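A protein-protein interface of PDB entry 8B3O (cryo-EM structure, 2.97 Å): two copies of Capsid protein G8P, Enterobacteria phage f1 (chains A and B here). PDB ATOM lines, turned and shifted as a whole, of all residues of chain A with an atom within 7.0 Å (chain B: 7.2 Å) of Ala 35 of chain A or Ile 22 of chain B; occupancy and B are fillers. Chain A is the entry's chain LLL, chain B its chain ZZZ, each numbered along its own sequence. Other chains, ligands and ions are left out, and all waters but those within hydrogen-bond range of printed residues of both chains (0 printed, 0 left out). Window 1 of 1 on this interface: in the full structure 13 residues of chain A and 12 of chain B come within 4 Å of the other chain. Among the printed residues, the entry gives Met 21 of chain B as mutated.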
ATOM      1  N   VAL A  29       8.682 -30.524   0.432  1.00  0.00           N
ATOM      2  CA  VAL A  29       7.563 -30.189  -0.442  1.00  0.00           C
ATOM      3  C   VAL A  29       7.304 -28.681  -0.416  1.00  0.00           C
ATOM      4  O   VAL A  29       6.962 -28.113  -1.448  1.00  0.00           O
ATOM      5  CB  VAL A  29       6.297 -31.027  -0.150  1.00  0.00           C
ATOM      6  CG1 VAL A  29       5.118 -30.647  -1.038  1.00  0.00           C
ATOM      7  CG2 VAL A  29       6.568 -32.519  -0.276  1.00  0.00           C
ATOM      8  N   VAL A  30       7.526 -28.036   0.740  1.00  0.00           N
ATOM      9  CA  VAL A  30       7.195 -26.627   0.931  1.00  0.00           C
ATOM     10  C   VAL A  30       8.261 -25.736   0.284  1.00  0.00           C
ATOM     11  O   VAL A  30       7.992 -24.574  -0.025  1.00  0.00           O
ATOM     12  CB  VAL A  30       6.964 -26.279   2.418  1.00  0.00           C
ATOM     13  CG1 VAL A  30       6.348 -24.899   2.605  1.00  0.00           C
ATOM     14  CG2 VAL A  30       6.108 -27.321   3.122  1.00  0.00           C
ATOM     15  N   VAL A  31       9.470 -26.281   0.090  1.00  0.00           N
ATOM     16  CA  VAL A  31      10.556 -25.563  -0.561  1.00  0.00           C
ATOM     17  C   VAL A  31      10.320 -25.559  -2.073  1.00  0.00           C
ATOM     18  O   VAL A  31      10.488 -24.524  -2.715  1.00  0.00           O
ATOM     19  CB  VAL A  31      11.940 -26.126  -0.166  1.00  0.00           C
ATOM     20  CG1 VAL A  31      13.082 -25.490  -0.946  1.00  0.00           C
ATOM     21  CG2 VAL A  31      12.202 -26.000   1.327  1.00  0.00           C
ATOM     22  N   ILE A  32       9.904 -26.711  -2.620  1.00  0.00           N
ATOM     23  CA  ILE A  32       9.776 -26.907  -4.059  1.00  0.00           C
ATOM     24  C   ILE A  32       8.482 -26.272  -4.573  1.00  0.00           C
ATOM     25  O   ILE A  32       8.509 -25.589  -5.598  1.00  0.00           O
ATOM     26  CB  ILE A  32       9.923 -28.396  -4.454  1.00  0.00           C
ATOM     27  CG1 ILE A  32      11.278 -28.959  -4.013  1.00  0.00           C
ATOM     28  CG2 ILE A  32       9.698 -28.596  -5.951  1.00  0.00           C
ATOM     29  CD1 ILE A  32      11.441 -30.453  -4.210  1.00  0.00           C
ATOM     30  N   VAL A  33       7.362 -26.499  -3.870  1.00  0.00           N
ATOM     31  CA  VAL A  33       6.071 -25.954  -4.280  1.00  0.00           C
ATOM     32  C   VAL A  33       6.116 -24.429  -4.183  1.00  0.00           C
ATOM     33  O   VAL A  33       5.571 -23.743  -5.046  1.00  0.00           O
ATOM     34  CB  VAL A  33       4.887 -26.591  -3.516  1.00  0.00           C
ATOM     35  CG1 VAL A  33       3.589 -25.800  -3.612  1.00  0.00           C
ATOM     36  CG2 VAL A  33       4.648 -28.032  -3.947  1.00  0.00           C
ATOM     37  N   GLY A  34       6.804 -23.918  -3.151  1.00  0.00           N
ATOM     38  CA  GLY A  34       7.047 -22.493  -2.991  1.00  0.00           C
ATOM     39  C   GLY A  34       7.636 -21.877  -4.258  1.00  0.00           C
ATOM     40  O   GLY A  34       7.056 -20.948  -4.818  1.00  0.00           O
ATOM     41  N   ALA A  35       8.760 -22.446  -4.715  1.00  0.00           N
ATOM     42  CA  ALA A  35       9.504 -21.970  -5.873  1.00  0.00           C
ATOM     43  C   ALA A  35       8.617 -21.930  -7.116  1.00  0.00           C
ATOM     44  O   ALA A  35       8.593 -20.920  -7.816  1.00  0.00           O
ATOM     45  CB  ALA A  35      10.717 -22.837  -6.096  1.00  0.00           C
ATOM     46  N   THR A  36       7.877 -23.023  -7.354  1.00  0.00           N
ATOM     47  CA  THR A  36       7.089 -23.212  -8.565  1.00  0.00           C
ATOM     48  C   THR A  36       5.984 -22.161  -8.648  1.00  0.00           C
ATOM     49  O   THR A  36       5.733 -21.603  -9.714  1.00  0.00           O
ATOM     50  CB  THR A  36       6.546 -24.647  -8.642  1.00  0.00           C
ATOM     51  OG1 THR A  36       7.605 -25.539  -8.291  1.00  0.00           O
ATOM     52  CG2 THR A  36       5.986 -25.018  -9.997  1.00  0.00           C
ATOM     53  N   ILE A  37       5.318 -21.903  -7.513  1.00  0.00           N
ATOM     54  CA  ILE A  37       4.176 -20.999  -7.470  1.00  0.00           C
ATOM     55  C   ILE A  37       4.661 -19.554  -7.367  1.00  0.00           C
ATOM     56  O   ILE A  37       3.856 -18.632  -7.434  1.00  0.00           O
ATOM     57  CB  ILE A  37       3.201 -21.396  -6.337  1.00  0.00           C
ATOM     58  CG1 ILE A  37       2.519 -22.737  -6.640  1.00  0.00           C
ATOM     59  CG2 ILE A  37       2.187 -20.290  -6.058  1.00  0.00           C
ATOM     60  CD1 ILE A  37       1.758 -23.346  -5.497  1.00  0.00           C
ATOM     61  N   GLY A  38       5.966 -19.370  -7.162  1.00  0.00           N
ATOM     62  CA  GLY A  38       6.585 -18.053  -7.144  1.00  0.00           C
ATOM     63  C   GLY A  38       7.040 -17.608  -8.532  1.00  0.00           C
ATOM     64  O   GLY A  38       7.121 -16.408  -8.793  1.00  0.00           O
ATOM     65  N   ILE A  39       7.373 -18.582  -9.393  1.00  0.00           N
ATOM     66  CA  ILE A  39       7.763 -18.300 -10.767  1.00  0.00           C
ATOM     67  C   ILE A  39       6.500 -18.053 -11.592  1.00  0.00           C
ATOM     68  O   ILE A  39       6.514 -17.228 -12.502  1.00  0.00           O
ATOM     69  CB  ILE A  39       8.678 -19.404 -11.354  1.00  0.00           C
ATOM     70  CG1 ILE A  39       9.978 -19.550 -10.554  1.00  0.00           C
ATOM     71  CG2 ILE A  39       8.960 -19.168 -12.838  1.00  0.00           C
ATOM     72  CD1 ILE A  39      10.844 -20.733 -10.952  1.00  0.00           C
ATOM     73  N   LYS A  40       5.408 -18.747 -11.241  1.00  0.00           N
ATOM     74  CA  LYS A  40       4.153 -18.665 -11.975  1.00  0.00           C
ATOM     75  C   LYS A  40       3.507 -17.295 -11.772  1.00  0.00           C
ATOM     76  O   LYS A  40       3.084 -16.658 -12.739  1.00  0.00           O
ATOM     77  CB  LYS A  40       3.216 -19.804 -11.562  1.00  0.00           C
ATOM     78  CG  LYS A  40       1.857 -19.814 -12.251  1.00  0.00           C
ATOM     79  CD  LYS A  40       1.131 -21.131 -12.151  1.00  0.00           C
ATOM     80  CE  LYS A  40       1.508 -22.093 -13.255  1.00  0.00           C
ATOM     81  NZ  LYS A  40       0.401 -23.031 -13.538  1.00  0.00           N
ATOM     82  N   GLN B  15      17.748 -31.640   0.330  1.00  0.00           N
ATOM     83  CA  GLN B  15      17.133 -30.332   0.505  1.00  0.00           C
ATOM     84  C   GLN B  15      18.145 -29.245   0.153  1.00  0.00           C
ATOM     85  O   GLN B  15      17.795 -28.277  -0.520  1.00  0.00           O
ATOM     86  CB  GLN B  15      16.567 -30.152   1.915  1.00  0.00           C
ATOM     87  CG  GLN B  15      15.643 -28.948   2.047  1.00  0.00           C
ATOM     88  CD  GLN B  15      14.671 -29.064   3.197  1.00  0.00           C
ATOM     89  OE1 GLN B  15      14.070 -30.110   3.432  1.00  0.00           O
ATOM     90  NE2 GLN B  15      14.495 -27.969   3.919  1.00  0.00           N
ATOM     91  N   SER B  17      20.659 -29.439  -1.913  1.00  0.00           N
ATOM     92  CA  SER B  17      20.825 -29.468  -3.358  1.00  0.00           C
ATOM     93  C   SER B  17      19.678 -28.734  -4.048  1.00  0.00           C
ATOM     94  O   SER B  17      19.921 -27.967  -4.975  1.00  0.00           O
ATOM     95  CB  SER B  17      20.955 -30.881  -3.864  1.00  0.00           C
ATOM     96  OG  SER B  17      21.879 -31.611  -3.072  1.00  0.00           O
ATOM     97  N   ALA B  18      18.444 -28.965  -3.573  1.00  0.00           N
ATOM     98  CA  ALA B  18      17.248 -28.357  -4.137  1.00  0.00           C
ATOM     99  C   ALA B  18      17.309 -26.834  -4.024  1.00  0.00           C
ATOM    100  O   ALA B  18      16.999 -26.139  -4.989  1.00  0.00           O
ATOM    101  CB  ALA B  18      16.010 -28.924  -3.482  1.00  0.00           C
ATOM    102  N   THR B  19      17.739 -26.333  -2.857  1.00  0.00           N
ATOM    103  CA  THR B  19      17.829 -24.903  -2.589  1.00  0.00           C
ATOM    104  C   THR B  19      18.779 -24.238  -3.588  1.00  0.00           C
ATOM    105  O   THR B  19      18.493 -23.146  -4.074  1.00  0.00           O
ATOM    106  CB  THR B  19      18.174 -24.625  -1.118  1.00  0.00           C
ATOM    107  OG1 THR B  19      17.175 -25.260  -0.319  1.00  0.00           O
ATOM    108  CG2 THR B  19      18.216 -23.153  -0.769  1.00  0.00           C
ATOM    109  N   GLU B  20      19.894 -24.917  -3.897  1.00  0.00           N
ATOM    110  CA  GLU B  20      20.884 -24.409  -4.835  1.00  0.00           C
ATOM    111  C   GLU B  20      20.262 -24.214  -6.217  1.00  0.00           C
ATOM    112  O   GLU B  20      20.547 -23.215  -6.873  1.00  0.00           O
ATOM    113  CB  GLU B  20      22.100 -25.334  -4.915  1.00  0.00           C
ATOM    114  CG  GLU B  20      22.944 -25.353  -3.650  1.00  0.00           C
ATOM    115  CD  GLU B  20      23.647 -26.669  -3.359  1.00  0.00           C
ATOM    116  OE1 GLU B  20      23.988 -27.393  -4.319  1.00  0.00           O
ATOM    117  OE2 GLU B  20      23.848 -26.973  -2.167  1.00  0.00           O
ATOM    118  N   MET B  21      19.408 -25.162  -6.636  1.00  0.00           N
ATOM    119  CA  MET B  21      18.854 -25.196  -7.984  1.00  0.00           C
ATOM    120  C   MET B  21      17.810 -24.095  -8.172  1.00  0.00           C
ATOM    121  O   MET B  21      17.688 -23.549  -9.267  1.00  0.00           O
ATOM    122  CB  MET B  21      18.221 -26.554  -8.306  1.00  0.00           C
ATOM    123  CG  MET B  21      19.230 -27.684  -8.389  1.00  0.00           C
ATOM    124  SD  MET B  21      18.775 -28.906  -9.641  1.00  0.00           S
ATOM    125  CE  MET B  21      19.238 -28.039 -11.142  1.00  0.00           C
ATOM    126  N   ILE B  22      17.069 -23.771  -7.103  1.00  0.00           N
ATOM    127  CA  ILE B  22      16.022 -22.757  -7.157  1.00  0.00           C
ATOM    128  C   ILE B  22      16.667 -21.379  -7.329  1.00  0.00           C
ATOM    129  O   ILE B  22      16.061 -20.474  -7.902  1.00  0.00           O
ATOM    130  CB  ILE B  22      15.091 -22.859  -5.927  1.00  0.00           C
ATOM    131  CG1 ILE B  22      14.433 -24.241  -5.844  1.00  0.00           C
ATOM    132  CG2 ILE B  22      14.052 -21.741  -5.901  1.00  0.00           C
ATOM    133  CD1 ILE B  22      13.913 -24.610  -4.472  1.00  0.00           C
ATOM    134  N   GLY B  23      17.910 -21.250  -6.849  1.00  0.00           N
ATOM    135  CA  GLY B  23      18.695 -20.037  -6.998  1.00  0.00           C
ATOM    136  C   GLY B  23      19.048 -19.782  -8.460  1.00  0.00           C
ATOM    137  O   GLY B  23      18.886 -18.666  -8.953  1.00  0.00           O
ATOM    138  N   TYR B  24      19.507 -20.841  -9.140  1.00  0.00           N
ATOM    139  CA  TYR B  24      19.900 -20.754 -10.536  1.00  0.00           C
ATOM    140  C   TYR B  24      18.675 -20.457 -11.399  1.00  0.00           C
ATOM    141  O   TYR B  24      18.785 -19.740 -12.389  1.00  0.00           O
ATOM    142  CB  TYR B  24      20.617 -22.024 -11.012  1.00  0.00           C
ATOM    143  CG  TYR B  24      21.778 -22.505 -10.174  1.00  0.00           C
ATOM    144  CD1 TYR B  24      22.692 -21.621  -9.613  1.00  0.00           C
ATOM    145  CD2 TYR B  24      21.985 -23.863  -9.972  1.00  0.00           C
ATOM    146  CE1 TYR B  24      23.760 -22.072  -8.849  1.00  0.00           C
ATOM    147  CE2 TYR B  24      23.052 -24.331  -9.218  1.00  0.00           C
ATOM    148  CZ  TYR B  24      23.941 -23.431  -8.653  1.00  0.00           C
ATOM    149  OH  TYR B  24      24.992 -23.882  -7.908  1.00  0.00           O
ATOM    150  N   ALA B  25      17.514 -20.986 -10.984  1.00  0.00           N
ATOM    151  CA  ALA B  25      16.287 -20.884 -11.760  1.00  0.00           C
ATOM    152  C   ALA B  25      15.693 -19.480 -11.658  1.00  0.00           C
ATOM    153  O   ALA B  25      15.161 -18.966 -12.642  1.00  0.00           O
ATOM    154  CB  ALA B  25      15.300 -21.946 -11.338  1.00  0.00           C
ATOM    155  N   TRP B  26      15.787 -18.864 -10.472  1.00  0.00           N
ATOM    156  CA  TRP B  26      15.290 -17.510 -10.288  1.00  0.00           C
ATOM    157  C   TRP B  26      16.063 -16.542 -11.182  1.00  0.00           C
ATOM    158  O   TRP B  26      15.472 -15.644 -11.776  1.00  0.00           O
ATOM    159  CB  TRP B  26      15.303 -17.094  -8.809  1.00  0.00           C
ATOM    160  CG  TRP B  26      13.977 -17.250  -8.123  1.00  0.00           C
ATOM    161  CD1 TRP B  26      13.657 -18.147  -7.145  1.00  0.00           C
ATOM    162  CD2 TRP B  26      12.782 -16.483  -8.364  1.00  0.00           C
ATOM    163  NE1 TRP B  26      12.351 -17.995  -6.762  1.00  0.00           N
ATOM    164  CE2 TRP B  26      11.788 -16.982  -7.492  1.00  0.00           C
ATOM    165  CE3 TRP B  26      12.452 -15.429  -9.228  1.00  0.00           C
ATOM    166  CZ2 TRP B  26      10.493 -16.460  -7.460  1.00  0.00           C
ATOM    167  CZ3 TRP B  26      11.173 -14.914  -9.197  1.00  0.00           C
ATOM    168  CH2 TRP B  26      10.209 -15.424  -8.323  1.00  0.00           C
ATOM    169  N   ALA B  27      17.373 -16.791 -11.328  1.00  0.00           N
ATOM    170  CA  ALA B  27      18.257 -15.961 -12.133  1.00  0.00           C
ATOM    171  C   ALA B  27      17.785 -15.922 -13.587  1.00  0.00           C
ATOM    172  O   ALA B  27      17.623 -14.843 -14.150  1.00  0.00           O
ATOM    173  CB  ALA B  27      19.682 -16.446 -12.011  1.00  0.00           C
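OG1 of Thr 19 of chain B is in hydrogen-bond range of O of Gln 15 of chain B.
No position is printed for both chains.
Of the 4 pairs that touch across the chains among the printed residues, none has its exchanged pair printed and touching as well.
Among the printed residues, merely in contact across the chains: Val 31 of chain A with Gln 15 of chain B, Val 31 of chain A with Ile 22 of chain B, Ala 35 of chain A with Ile 22 of chain B and Gly 38 of chain A with Trp 26 of chain B.
Ala 35 of chain A touches just one residue of chain B: Ile 22.
Ile 22 of chain B touches two residues of chain A.
No residue of chain B comes within 4 Å of Gly 34 of chain A.
Of the printed residues of chain A, Gln 15 of chain B touches Val 31.
Printed residues of chain A within 4 Å of Trp 26 of chain B: Gly 38.
Of the printed residues of chain B, Gly 38 of chain A touches Trp 26 (3.3 Å).
Of the printed residues of chain B, Val 31 of chain A touches Gln 15 (3.98 Å) and Ile 22 (3.7 Å).
Tyr 24 of chain B touches none of the printed residues of chain A.
Ile 39 of chain A touches none of the printed residues of chain B.
Of the 12 printed residues of chain B, 3 touch a printed residue of chain A.
Printed residues of chain B that touch a printed residue of chain A: Gln 15, Ile 22 and Trp 26.
Hydrophobic or aromatic side chains of chain B that line the printed part of chain A: Ile 22 and Trp 26.
Of the 12 printed residues of chain A, 3 touch a printed residue of chain B.
Hydrophobic or aromatic side chains of chain A within 4 Å of the printed part of chain B: Val 31 and Ala 35.
Among the printed residues, 4 pairs touch across the chains.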
